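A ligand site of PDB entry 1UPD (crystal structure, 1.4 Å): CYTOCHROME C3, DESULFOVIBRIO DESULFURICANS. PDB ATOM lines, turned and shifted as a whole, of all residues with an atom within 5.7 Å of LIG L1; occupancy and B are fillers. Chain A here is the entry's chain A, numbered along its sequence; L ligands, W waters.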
ATOM      1  N   ALA A   1      17.883  10.332  10.108  1.00  0.00           N
ATOM      2  CA  ALA A   1      17.023  11.452  10.429  1.00  0.00           C
ATOM      3  C   ALA A   1      17.214  11.939  11.867  1.00  0.00           C
ATOM      4  O   ALA A   1      17.751  11.194  12.686  1.00  0.00           O
ATOM      5  CB  ALA A   1      15.553  11.062  10.244  1.00  0.00           C
ATOM      6  N   PRO A   2      16.744  13.118  12.187  1.00  0.00           N
ATOM      7  CA  PRO A   2      16.682  13.529  13.593  1.00  0.00           C
ATOM      8  C   PRO A   2      15.633  12.685  14.317  1.00  0.00           C
ATOM      9  O   PRO A   2      14.756  12.086  13.683  1.00  0.00           O
ATOM     10  CB  PRO A   2      16.158  14.979  13.503  1.00  0.00           C
ATOM     11  CG  PRO A   2      15.354  14.961  12.237  1.00  0.00           C
ATOM     12  CD  PRO A   2      16.196  14.151  11.286  1.00  0.00           C
ATOM     13  N   ALA A   3      15.742  12.628  15.619  1.00  0.00           N
ATOM     14  CA  ALA A   3      14.780  11.928  16.466  1.00  0.00           C
ATOM     15  C   ALA A   3      13.377  12.492  16.274  1.00  0.00           C
ATOM     16  O   ALA A   3      13.153  13.714  16.248  1.00  0.00           O
ATOM     17  CB  ALA A   3      15.096  12.085  17.948  1.00  0.00           C
ATOM     18  N   VAL A   4      12.394  11.604  16.161  1.00  0.00           N
ATOM     19  CA  VAL A   4      11.016  12.089  16.113  1.00  0.00           C
ATOM     20  C   VAL A   4      10.672  12.767  17.433  1.00  0.00           C
ATOM     21  O   VAL A   4      11.059  12.322  18.517  1.00  0.00           O
ATOM     22  CB  VAL A   4      10.030  10.936  15.804  1.00  0.00           C
ATOM     23  CG1 VAL A   4       9.928   9.975  16.988  1.00  0.00           C
ATOM     24  CG2 VAL A   4       8.650  11.459  15.443  1.00  0.00           C
ATOM     25  N   PRO A   5       9.975  13.905  17.449  1.00  0.00           N
ATOM     26  CA  PRO A   5       9.553  14.470  18.742  1.00  0.00           C
ATOM     27  C   PRO A   5       8.695  13.488  19.534  1.00  0.00           C
ATOM     28  O   PRO A   5       7.783  12.854  18.953  1.00  0.00           O
ATOM     29  CB  PRO A   5       8.766  15.716  18.335  1.00  0.00           C
ATOM     30  CG  PRO A   5       9.382  16.113  17.021  1.00  0.00           C
ATOM     31  CD  PRO A   5       9.679  14.779  16.308  1.00  0.00           C
ATOM     32  N   VAL A   9       4.135  18.985  19.616  1.00  0.00           N
ATOM     33  CA  VAL A   9       4.932  20.162  19.252  1.00  0.00           C
ATOM     34  C   VAL A   9       4.021  21.273  18.691  1.00  0.00           C
ATOM     35  O   VAL A   9       2.959  20.987  18.122  1.00  0.00           O
ATOM     36  CB  VAL A   9       6.033  19.850  18.235  1.00  0.00           C
ATOM     37  CG1 VAL A   9       7.076  18.883  18.832  1.00  0.00           C
ATOM     38  CG2 VAL A   9       5.491  19.314  16.904  1.00  0.00           C
ATOM     39  N   GLU A  10       4.435  22.532  18.844  1.00  0.00           N
ATOM     40  CA  GLU A  10       3.660  23.635  18.311  1.00  0.00           C
ATOM     41  C   GLU A  10       3.721  23.708  16.786  1.00  0.00           C
ATOM     42  O   GLU A  10       4.758  23.639  16.137  1.00  0.00           O
ATOM     43  CB  GLU A  10       4.210  24.971  18.790  1.00  0.00           C
ATOM     44  CG  GLU A  10       4.423  25.050  20.285  1.00  0.00           C
ATOM     45  CD  GLU A  10       5.437  26.156  20.559  1.00  0.00           C
ATOM     46  OE1 GLU A  10       6.646  26.105  20.222  1.00  0.00           O
ATOM     47  OE2 GLU A  10       4.951  27.137  21.162  1.00  0.00           O
ATOM     48  N   VAL A  11       2.568  23.926  16.181  1.00  0.00           N
ATOM     49  CA  VAL A  11       2.475  24.353  14.784  1.00  0.00           C
ATOM     50  C   VAL A  11       1.887  25.758  14.814  1.00  0.00           C
ATOM     51  O   VAL A  11       0.689  25.925  15.046  1.00  0.00           O
ATOM     52  CB  VAL A  11       1.630  23.417  13.888  1.00  0.00           C
ATOM     53  CG1 VAL A  11       1.812  23.805  12.402  1.00  0.00           C
ATOM     54  CG2 VAL A  11       2.028  21.960  14.083  1.00  0.00           C
ATOM     55  N   LYS A  12       2.750  26.748  14.640  1.00  0.00           N
ATOM     56  CA  LYS A  12       2.343  28.159  14.762  1.00  0.00           C
ATOM     57  C   LYS A  12       1.802  28.763  13.473  1.00  0.00           C
ATOM     58  O   LYS A  12       2.549  28.821  12.506  1.00  0.00           O
ATOM     59  CB  LYS A  12       3.548  28.986  15.236  1.00  0.00           C
ATOM     60  CG  LYS A  12       3.939  28.630  16.654  1.00  0.00           C
ATOM     61  CD  LYS A  12       4.975  29.631  17.173  1.00  0.00           C
ATOM     62  CE  LYS A  12       5.404  29.298  18.590  1.00  0.00           C
ATOM     63  NZ  LYS A  12       6.416  30.287  19.096  1.00  0.00           N
ATOM     64  N   PHE A  20       0.766  19.407  17.559  1.00  0.00           N
ATOM     65  CA  PHE A  20       0.767  18.241  16.690  1.00  0.00           C
ATOM     66  C   PHE A  20       1.431  17.067  17.431  1.00  0.00           C
ATOM     67  O   PHE A  20       2.604  17.211  17.825  1.00  0.00           O
ATOM     68  CB  PHE A  20       1.579  18.593  15.419  1.00  0.00           C
ATOM     69  CG  PHE A  20       1.832  17.328  14.608  1.00  0.00           C
ATOM     70  CD1 PHE A  20       0.778  16.776  13.870  1.00  0.00           C
ATOM     71  CD2 PHE A  20       3.058  16.670  14.591  1.00  0.00           C
ATOM     72  CE1 PHE A  20       0.961  15.601  13.157  1.00  0.00           C
ATOM     73  CE2 PHE A  20       3.233  15.490  13.873  1.00  0.00           C
ATOM     74  CZ  PHE A  20       2.172  14.976  13.161  1.00  0.00           C
ATOM     75  N   HIS A  22       3.135  13.479  17.368  1.00  0.00           N
ATOM     76  CA  HIS A  22       3.685  12.453  16.471  1.00  0.00           C
ATOM     77  C   HIS A  22       3.171  11.056  16.781  1.00  0.00           C
ATOM     78  O   HIS A  22       3.085  10.250  15.838  1.00  0.00           O
ATOM     79  CB  HIS A  22       5.223  12.482  16.486  1.00  0.00           C
ATOM     80  CG  HIS A  22       5.799  13.535  15.580  1.00  0.00           C
ATOM     81  ND1 HIS A  22       5.929  14.866  15.949  1.00  0.00           N
ATOM     82  CD2 HIS A  22       6.304  13.491  14.324  1.00  0.00           C
ATOM     83  CE1 HIS A  22       6.479  15.566  14.950  1.00  0.00           C
ATOM     84  NE2 HIS A  22       6.724  14.758  13.917  1.00  0.00           N
ATOM     85  N   HIS A  25       0.694   9.153  14.708  1.00  0.00           N
ATOM     86  CA  HIS A  25       1.147   9.141  13.336  1.00  0.00           C
ATOM     87  C   HIS A  25       2.325   8.216  13.166  1.00  0.00           C
ATOM     88  O   HIS A  25       2.979   8.218  12.100  1.00  0.00           O
ATOM     89  CB  HIS A  25       1.531  10.576  12.888  1.00  0.00           C
ATOM     90  CG  HIS A  25       0.339  11.495  12.950  1.00  0.00           C
ATOM     91  ND1 HIS A  25       0.171  12.315  14.036  1.00  0.00           N
ATOM     92  CD2 HIS A  25      -0.729  11.661  12.134  1.00  0.00           C
ATOM     93  CE1 HIS A  25      -0.971  13.004  13.888  1.00  0.00           C
ATOM     94  NE2 HIS A  25      -1.531  12.610  12.715  1.00  0.00           N
ATOM     95  N   VAL A  28       2.546   6.365   9.903  1.00  0.00           N
ATOM     96  CA  VAL A  28       2.658   7.215   8.709  1.00  0.00           C
ATOM     97  C   VAL A  28       4.129   7.370   8.383  1.00  0.00           C
ATOM     98  O   VAL A  28       4.914   7.700   9.304  1.00  0.00           O
ATOM     99  CB  VAL A  28       1.987   8.582   8.934  1.00  0.00           C
ATOM    100  CG1 VAL A  28       2.223   9.469   7.703  1.00  0.00           C
ATOM    101  CG2 VAL A  28       0.502   8.407   9.257  1.00  0.00           C
ATOM    102  N   GLU A  29       4.527   7.186   7.135  1.00  0.00           N
ATOM    103  CA  GLU A  29       5.927   7.412   6.785  1.00  0.00           C
ATOM    104  C   GLU A  29       6.322   8.858   7.105  1.00  0.00           C
ATOM    105  O   GLU A  29       5.540   9.759   6.798  1.00  0.00           O
ATOM    106  CB  GLU A  29       6.225   7.120   5.334  1.00  0.00           C
ATOM    107  CG  GLU A  29       5.993   5.680   4.909  1.00  0.00           C
ATOM    108  CD  GLU A  29       6.227   5.398   3.453  1.00  0.00           C
ATOM    109  OE1 GLU A  29       6.326   6.297   2.616  1.00  0.00           O
ATOM    110  OE2 GLU A  29       6.298   4.192   3.122  1.00  0.00           O
ATOM    111  N   CYS A  30       7.521   9.051   7.664  1.00  0.00           N
ATOM    112  CA  CYS A  30       7.928  10.450   7.910  1.00  0.00           C
ATOM    113  C   CYS A  30       7.816  11.330   6.670  1.00  0.00           C
ATOM    114  O   CYS A  30       7.385  12.490   6.721  1.00  0.00           O
ATOM    115  CB  CYS A  30       9.372  10.587   8.430  1.00  0.00           C
ATOM    116  SG  CYS A  30       9.947   9.441   9.665  1.00  0.00           S
ATOM    117  N   THR A  32       5.821  11.270   4.243  1.00  0.00           N
ATOM    118  CA  THR A  32       4.485  11.779   3.855  1.00  0.00           C
ATOM    119  C   THR A  32       4.328  13.253   4.196  1.00  0.00           C
ATOM    120  O   THR A  32       3.766  14.056   3.417  1.00  0.00           O
ATOM    121  CB  THR A  32       3.394  10.945   4.581  1.00  0.00           C
ATOM    122  OG1 THR A  32       3.512   9.616   4.087  1.00  0.00           O
ATOM    123  CG2 THR A  32       2.006  11.498   4.276  1.00  0.00           C
ATOM    124  N   CYS A  33       4.846  13.620   5.378  1.00  0.00           N
ATOM    125  CA  CYS A  33       4.708  14.998   5.865  1.00  0.00           C
ATOM    126  C   CYS A  33       5.987  15.796   5.612  1.00  0.00           C
ATOM    127  O   CYS A  33       5.966  16.880   5.044  1.00  0.00           O
ATOM    128  CB  CYS A  33       4.434  14.963   7.386  1.00  0.00           C
ATOM    129  SG  CYS A  33       2.899  14.033   7.638  1.00  0.00           S
ATOM    130  N   HIS A  34       7.105  15.240   6.037  1.00  0.00           N
ATOM    131  CA  HIS A  34       8.427  15.810   5.845  1.00  0.00           C
ATOM    132  C   HIS A  34       8.879  15.397   4.446  1.00  0.00           C
ATOM    133  O   HIS A  34       9.798  14.585   4.244  1.00  0.00           O
ATOM    134  CB  HIS A  34       9.380  15.318   6.926  1.00  0.00           C
ATOM    135  CG  HIS A  34       8.973  15.741   8.298  1.00  0.00           C
ATOM    136  ND1 HIS A  34       9.085  16.994   8.797  1.00  0.00           N
ATOM    137  CD2 HIS A  34       8.427  14.984   9.296  1.00  0.00           C
ATOM    138  CE1 HIS A  34       8.624  17.001  10.074  1.00  0.00           C
ATOM    139  NE2 HIS A  34       8.207  15.768  10.395  1.00  0.00           N
ATOM    140  N   TYR A  43      13.717  18.027   7.366  1.00  0.00           N
ATOM    141  CA  TYR A  43      12.797  17.998   8.518  1.00  0.00           C
ATOM    142  C   TYR A  43      12.611  19.380   9.116  1.00  0.00           C
ATOM    143  O   TYR A  43      12.209  19.493  10.299  1.00  0.00           O
ATOM    144  CB  TYR A  43      13.361  17.054   9.588  1.00  0.00           C
ATOM    145  CG  TYR A  43      13.352  15.627   9.124  1.00  0.00           C
ATOM    146  CD1 TYR A  43      14.381  15.121   8.330  1.00  0.00           C
ATOM    147  CD2 TYR A  43      12.297  14.808   9.484  1.00  0.00           C
ATOM    148  CE1 TYR A  43      14.364  13.802   7.899  1.00  0.00           C
ATOM    149  CE2 TYR A  43      12.280  13.513   9.052  1.00  0.00           C
ATOM    150  CZ  TYR A  43      13.301  13.012   8.269  1.00  0.00           C
ATOM    151  OH  TYR A  43      13.236  11.711   7.888  1.00  0.00           O
ATOM    152  N   ALA A  44      12.898  20.393   8.330  1.00  0.00           N
ATOM    153  CA  ALA A  44      12.732  21.771   8.752  1.00  0.00           C
ATOM    154  C   ALA A  44      11.260  22.085   9.019  1.00  0.00           C
ATOM    155  O   ALA A  44      10.346  21.448   8.492  1.00  0.00           O
ATOM    156  CB  ALA A  44      13.318  22.709   7.698  1.00  0.00           C
ATOM    157  N   LYS A  45      11.025  23.117   9.848  1.00  0.00           N
ATOM    158  CA  LYS A  45       9.652  23.503  10.165  1.00  0.00           C
ATOM    159  C   LYS A  45       8.911  23.843   8.869  1.00  0.00           C
ATOM    160  O   LYS A  45       9.505  24.475   8.013  1.00  0.00           O
ATOM    161  CB  LYS A  45       9.614  24.680  11.141  1.00  0.00           C
ATOM    162  CG  LYS A  45      10.047  24.237  12.534  1.00  0.00           C
ATOM    163  CD  LYS A  45      10.004  25.414  13.497  1.00  0.00           C
ATOM    164  CE  LYS A  45      10.356  25.018  14.931  1.00  0.00           C
ATOM    165  NZ  LYS A  45      10.779  26.268  15.639  1.00  0.00           N
ATOM    166  N   CYS A  46       7.648  23.441   8.766  1.00  0.00           N
ATOM    167  CA  CYS A  46       6.912  23.663   7.523  1.00  0.00           C
ATOM    168  C   CYS A  46       6.817  25.137   7.180  1.00  0.00           C
ATOM    169  O   CYS A  46       6.853  25.438   5.984  1.00  0.00           O
ATOM    170  CB  CYS A  46       5.491  23.097   7.594  1.00  0.00           C
ATOM    171  SG  CYS A  46       5.340  21.510   8.468  1.00  0.00           S
ATOM    172  N   GLY A  47       6.685  26.015   8.166  1.00  0.00           N
ATOM    173  CA  GLY A  47       6.572  27.425   7.893  1.00  0.00           C
ATOM    174  C   GLY A  47       7.917  28.141   7.851  1.00  0.00           C
ATOM    175  O   GLY A  47       7.971  29.390   7.877  1.00  0.00           O
HETATM  176 FE1  LIG L   1       7.502  15.256  12.153  1.00  0.00          FE
HETATM  177  C1  LIG L   1       8.011  18.360  13.533  1.00  0.00           C
HETATM  178  C2  LIG L   1      10.725  14.436  12.721  1.00  0.00           C
HETATM  179  C3  LIG L   1       6.836  12.034  11.159  1.00  0.00           C
HETATM  180  C4  LIG L   1       4.493  16.265  10.905  1.00  0.00           C
HETATM  181  N1  LIG L   1       9.018  16.194  13.009  1.00  0.00           N
HETATM  182  C5  LIG L   1       9.081  17.470  13.537  1.00  0.00           C
HETATM  183  C6  LIG L   1      10.415  17.714  14.024  1.00  0.00           C
HETATM  184  C7  LIG L   1      11.174  16.639  13.760  1.00  0.00           C
HETATM  185  C8  LIG L   1      10.302  15.685  13.120  1.00  0.00           C
HETATM  186  C9  LIG L   1      12.659  16.446  14.014  1.00  0.00           C
HETATM  187  C10 LIG L   1      10.895  19.022  14.639  1.00  0.00           C
HETATM  188  C11 LIG L   1      11.208  20.060  13.521  1.00  0.00           C
HETATM  189  C12 LIG L   1      11.813  21.342  14.061  1.00  0.00           C
HETATM  190  O1  LIG L   1      11.252  21.860  15.052  1.00  0.00           O
HETATM  191  O2  LIG L   1      12.834  21.810  13.483  1.00  0.00           O
HETATM  192  N2  LIG L   1       8.534  13.556  12.042  1.00  0.00           N
HETATM  193  C13 LIG L   1       9.897  13.430  12.254  1.00  0.00           C
HETATM  194  C14 LIG L   1      10.329  12.086  11.975  1.00  0.00           C
HETATM  195  C15 LIG L   1       9.237  11.391  11.583  1.00  0.00           C
HETATM  196  C16 LIG L   1       8.137  12.331  11.591  1.00  0.00           C
HETATM  197  C17 LIG L   1      11.790  11.605  12.119  1.00  0.00           C
HETATM  198  C18 LIG L   1       9.082   9.929  11.195  1.00  0.00           C
HETATM  199  C19 LIG L   1       9.580   8.983  12.300  1.00  0.00           C
HETATM  200  N3  LIG L   1       5.977  14.330  11.276  1.00  0.00           N
HETATM  201  C20 LIG L   1       5.879  12.990  10.925  1.00  0.00           C
HETATM  202  C21 LIG L   1       4.630  12.739  10.234  1.00  0.00           C
HETATM  203  C22 LIG L   1       4.008  13.913  10.142  1.00  0.00           C
HETATM  204  C23 LIG L   1       4.826  14.914  10.797  1.00  0.00           C
HETATM  205  C24 LIG L   1       4.227  11.317   9.741  1.00  0.00           C
HETATM  206  C25 LIG L   1       2.681  14.248   9.455  1.00  0.00           C
HETATM  207  C26 LIG L   1       1.496  13.361   9.868  1.00  0.00           C
HETATM  208  N4  LIG L   1       6.469  16.939  12.233  1.00  0.00           N
HETATM  209  C27 LIG L   1       5.230  17.176  11.632  1.00  0.00           C
HETATM  210  C28 LIG L   1       4.834  18.532  11.904  1.00  0.00           C
HETATM  211  C29 LIG L   1       5.779  19.115  12.679  1.00  0.00           C
HETATM  212  C30 LIG L   1       6.813  18.145  12.874  1.00  0.00           C
HETATM  213  C31 LIG L   1       3.518  19.169  11.431  1.00  0.00           C
HETATM  214  C32 LIG L   1       5.760  20.549  13.238  1.00  0.00           C
HETATM  215  C33 LIG L   1       6.505  21.435  12.211  1.00  0.00           C
HETATM  216  C34 LIG L   1       6.408  22.924  12.396  1.00  0.00           C
HETATM  217  O3  LIG L   1       6.195  23.411  13.505  1.00  0.00           O
HETATM  218  O4  LIG L   1       6.603  23.646  11.398  1.00  0.00           O
HETATM  219 FE1  LG2 L   2      -3.312  13.169  12.029  1.00  0.00          FE
HETATM  220  C1  LG2 L   2      -4.710  11.538  14.672  1.00  0.00           C
HETATM  221  C2  LG2 L   2      -3.269  16.087  13.887  1.00  0.00           C
HETATM  222  C3  LG2 L   2      -1.706  14.748   9.485  1.00  0.00           C
HETATM  223  C4  LG2 L   2      -3.415  10.298  10.173  1.00  0.00           C
HETATM  224  N1  LG2 L   2      -3.857  13.692  13.878  1.00  0.00           N
HETATM  225  C5  LG2 L   2      -4.439  12.890  14.822  1.00  0.00           C
HETATM  226  C6  LG2 L   2      -4.802  13.663  15.997  1.00  0.00           C
HETATM  227  C7  LG2 L   2      -4.374  14.931  15.807  1.00  0.00           C
HETATM  228  C8  LG2 L   2      -3.795  14.953  14.467  1.00  0.00           C
HETATM  229  C9  LG2 L   2      -4.445  16.184  16.681  1.00  0.00           C
HETATM  230  C10 LG2 L   2      -5.642  13.114  17.175  1.00  0.00           C
HETATM  231  C11 LG2 L   2      -4.772  12.509  18.260  1.00  0.00           C
HETATM  232  C12 LG2 L   2      -5.513  12.356  19.585  1.00  0.00           C
HETATM  233  O1  LG2 L   2      -5.932  13.400  20.145  1.00  0.00           O
HETATM  234  O2  LG2 L   2      -5.629  11.221  20.065  1.00  0.00           O
HETATM  235  N2  LG2 L   2      -2.652  15.012  11.731  1.00  0.00           N
HETATM  236  C13 LG2 L   2      -2.743  16.111  12.599  1.00  0.00           C
HETATM  237  C14 LG2 L   2      -2.190  17.285  11.976  1.00  0.00           C
HETATM  238  C15 LG2 L   2      -1.728  16.912  10.780  1.00  0.00           C
HETATM  239  C16 LG2 L   2      -2.020  15.507  10.601  1.00  0.00           C
HETATM  240  C17 LG2 L   2      -2.159  18.714  12.584  1.00  0.00           C
HETATM  241  C18 LG2 L   2      -1.026  17.713   9.702  1.00  0.00           C
HETATM  242  C19 LG2 L   2       0.213  18.519  10.154  1.00  0.00           C
HETATM  243  N3  LG2 L   2      -2.730  12.654  10.196  1.00  0.00           N
HETATM  244  C20 LG2 L   2      -2.089  13.447   9.288  1.00  0.00           C
HETATM  245  C21 LG2 L   2      -1.837  12.716   8.052  1.00  0.00           C
HETATM  246  C22 LG2 L   2      -2.342  11.479   8.219  1.00  0.00           C
HETATM  247  C23 LG2 L   2      -2.874  11.423   9.571  1.00  0.00           C
HETATM  248  C24 LG2 L   2      -1.144  13.392   6.872  1.00  0.00           C
HETATM  249  C25 LG2 L   2      -2.497  10.274   7.263  1.00  0.00           C
HETATM  250  C26 LG2 L   2      -1.436  10.211   6.160  1.00  0.00           C
HETATM  251  N4  LG2 L   2      -3.962  11.302  12.354  1.00  0.00           N
HETATM  252  C27 LG2 L   2      -3.894  10.240  11.473  1.00  0.00           C
HETATM  253  C28 LG2 L   2      -4.333   9.036  12.117  1.00  0.00           C
HETATM  254  C29 LG2 L   2      -4.692   9.370  13.386  1.00  0.00           C
HETATM  255  C30 LG2 L   2      -4.469  10.801  13.532  1.00  0.00           C
HETATM  256  C31 LG2 L   2      -4.321   7.645  11.461  1.00  0.00           C
HETATM  257  C32 LG2 L   2      -5.213   8.430  14.460  1.00  0.00           C
HETATM  258  C33 LG2 L   2      -6.709   8.113  14.208  1.00  0.00           C
HETATM  259  C34 LG2 L   2      -7.151   6.954  15.098  1.00  0.00           C
HETATM  260  O3  LG2 L   2      -7.088   7.150  16.325  1.00  0.00           O
HETATM  261  O4  LG2 L   2      -7.554   5.931  14.494  1.00  0.00           O
HETATM  262 FE1  LG3 L   3       6.056  21.475   1.840  1.00  0.00          FE
HETATM  263  C1  LG3 L   3       4.654  21.296  -1.259  1.00  0.00           C
HETATM  264  C2  LG3 L   3       3.291  20.175   3.215  1.00  0.00           C
HETATM  265  C3  LG3 L   3       7.690  21.226   4.871  1.00  0.00           C
HETATM  266  C4  LG3 L   3       8.743  23.150   0.546  1.00  0.00           C
HETATM  267  N1  LG3 L   3       4.326  20.852   1.121  1.00  0.00           N
HETATM  268  C5  LG3 L   3       3.887  20.873  -0.174  1.00  0.00           C
HETATM  269  C6  LG3 L   3       2.514  20.430  -0.238  1.00  0.00           C
HETATM  270  C7  LG3 L   3       2.141  20.045   0.998  1.00  0.00           C
HETATM  271  C8  LG3 L   3       3.262  20.365   1.871  1.00  0.00           C
HETATM  272  C9  LG3 L   3       0.845  19.400   1.516  1.00  0.00           C
HETATM  273  C10 LG3 L   3       1.686  20.416  -1.533  1.00  0.00           C
HETATM  274  C11 LG3 L   3       1.210  21.861  -1.826  1.00  0.00           C
HETATM  275  C12 LG3 L   3       0.482  21.991  -3.164  1.00  0.00           C
HETATM  276  O1  LG3 L   3       0.352  20.991  -3.865  1.00  0.00           O
HETATM  277  O2  LG3 L   3       0.073  23.139  -3.450  1.00  0.00           O
HETATM  278  N2  LG3 L   3       5.599  20.868   3.679  1.00  0.00           N
HETATM  279  C13 LG3 L   3       4.352  20.378   4.076  1.00  0.00           C
HETATM  280  C14 LG3 L   3       4.326  20.135   5.504  1.00  0.00           C
HETATM  281  C15 LG3 L   3       5.563  20.426   5.947  1.00  0.00           C
HETATM  282  C16 LG3 L   3       6.362  20.864   4.833  1.00  0.00           C
HETATM  283  C17 LG3 L   3       3.080  19.706   6.290  1.00  0.00           C
HETATM  284  C18 LG3 L   3       6.129  20.347   7.359  1.00  0.00           C
HETATM  285  C19 LG3 L   3       5.960  18.943   7.978  1.00  0.00           C
HETATM  286  N3  LG3 L   3       7.815  22.093   2.554  1.00  0.00           N
HETATM  287  C20 LG3 L   3       8.339  21.856   3.816  1.00  0.00           C
HETATM  288  C21 LG3 L   3       9.639  22.462   3.916  1.00  0.00           C
HETATM  289  C22 LG3 L   3       9.885  23.121   2.760  1.00  0.00           C
HETATM  290  C23 LG3 L   3       8.810  22.796   1.876  1.00  0.00           C
HETATM  291  C24 LG3 L   3      10.460  22.401   5.200  1.00  0.00           C
HETATM  292  C25 LG3 L   3      11.020  24.101   2.428  1.00  0.00           C
HETATM  293  C26 LG3 L   3      12.398  23.429   2.463  1.00  0.00           C
HETATM  294  N4  LG3 L   3       6.554  22.135   0.037  1.00  0.00           N
HETATM  295  C27 LG3 L   3       7.733  22.762  -0.311  1.00  0.00           C
HETATM  296  C28 LG3 L   3       7.790  22.988  -1.736  1.00  0.00           C
HETATM  297  C29 LG3 L   3       6.657  22.468  -2.258  1.00  0.00           C
HETATM  298  C30 LG3 L   3       5.876  21.915  -1.166  1.00  0.00           C
HETATM  299  C31 LG3 L   3       9.001  23.665  -2.403  1.00  0.00           C
HETATM  300  C32 LG3 L   3       6.229  22.416  -3.718  1.00  0.00           C
HETATM  301  C33 LG3 L   3       6.785  21.189  -4.463  1.00  0.00           C
HETATM  302  C34 LG3 L   3       6.377  19.847  -3.914  1.00  0.00           C
HETATM  303  O3  LG3 L   3       7.263  19.220  -3.286  1.00  0.00           O
HETATM  304  O4  LG3 L   3       5.219  19.452  -4.128  1.00  0.00           O
HETATM  305  O   HOH W   1       6.146  26.068  10.629  1.00  0.00           O
HETATM  306  O   HOH W   2       9.405  20.053  10.723  1.00  0.00           O
HETATM  307  O   HOH W   3       8.577  21.566  15.226  1.00  0.00           O
HETATM  308  O   HOH W   4       5.625  25.963  13.936  1.00  0.00           O
HETATM  309  O   HOH W   5       5.983   8.738  11.674  1.00  0.00           O
HETATM  310  O   HOH W   6       7.349  23.498  16.600  1.00  0.00           O
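The side-chain sulfur (SG) of Cys 30 is bonded to a carbon (C18) of LIG L1 (1.8 Å).
The side-chain sulfur (SG) of Cys 33 is covalently linked to a carbon (C25) of LIG L1, 1.8 Å away.
A ring nitrogen (NE2) of His 34 is bound to an iron atom (FE1) of LIG L1 (2.0 Å).
An iron atom (FE1) of LIG L1 is bound by a ring nitrogen (NE2) of His 22.
An oxygen (O4) of LIG L1 sits at hydrogen-bond distance from the backbone NH of Cys 46 (2.8 Å).
The backbone carbonyl oxygen of Glu 10 sits close to an oxygen (O3) of LIG L1.
An iron atom (FE1) of LG2 L2 is bound by a ring nitrogen (NE2) of His 25 (2.0 Å).
The side-chain sulfur (SG) of Cys 46 is covalently linked to a carbon (C18) of LG3 L3 (1.8 Å).
N of Phe 20 is in hydrogen-bond range of O of Val 9, 2.8 Å away.
OG1 of Thr 32 lies close to O of Glu 29 (3.4 Å).
Pro 2 touches LIG L1.
Ala 3 touches LIG L1 (O to C9, 3.6 Å).
Val 4 touches LIG L1.
Pro 5 touches LIG L1.
Val 9 touches LIG L1 (CG2 to C32, 3.9 Å).
Phe 20 touches LIG L1.
His 25 touches LIG L1.
CG1 of Val 28 touches C24 of LIG L1 (3.4 Å).
Glu 29 touches LIG L1 (O to C24, 3.6 Å).
O of Tyr 43 touches C11 of LIG L1, 3.4 Å away.
Lys 45 touches LIG L1.
Within 4 Å of LIG L1: Pro 2, Ala 3, Val 4, Pro 5, Val 9, Glu 10, Phe 20, His 22, His 25, Val 28, Glu 29, Cys 30, Cys 33, His 34, Tyr 43, Lys 45 and Cys 46.
The nearest printed residue that does not touch LIG L1 is Gly 47 (4.01 Å).
Water W1 bridges the backbone NH of Gly 47 (2.5 Å) and an oxygen (O4) of LIG L1 (2.6 Å).
Water W4 lies within hydrogen-bond range of O3 of LIG L1 (2.7 Å), N of Lys 12 (3.1 Å) and O of Glu 10 (3.3 Å).
Water W6 lies within hydrogen-bond range of O of Glu 10 (2.6 Å) and O3 of LIG L1 (3.3 Å).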
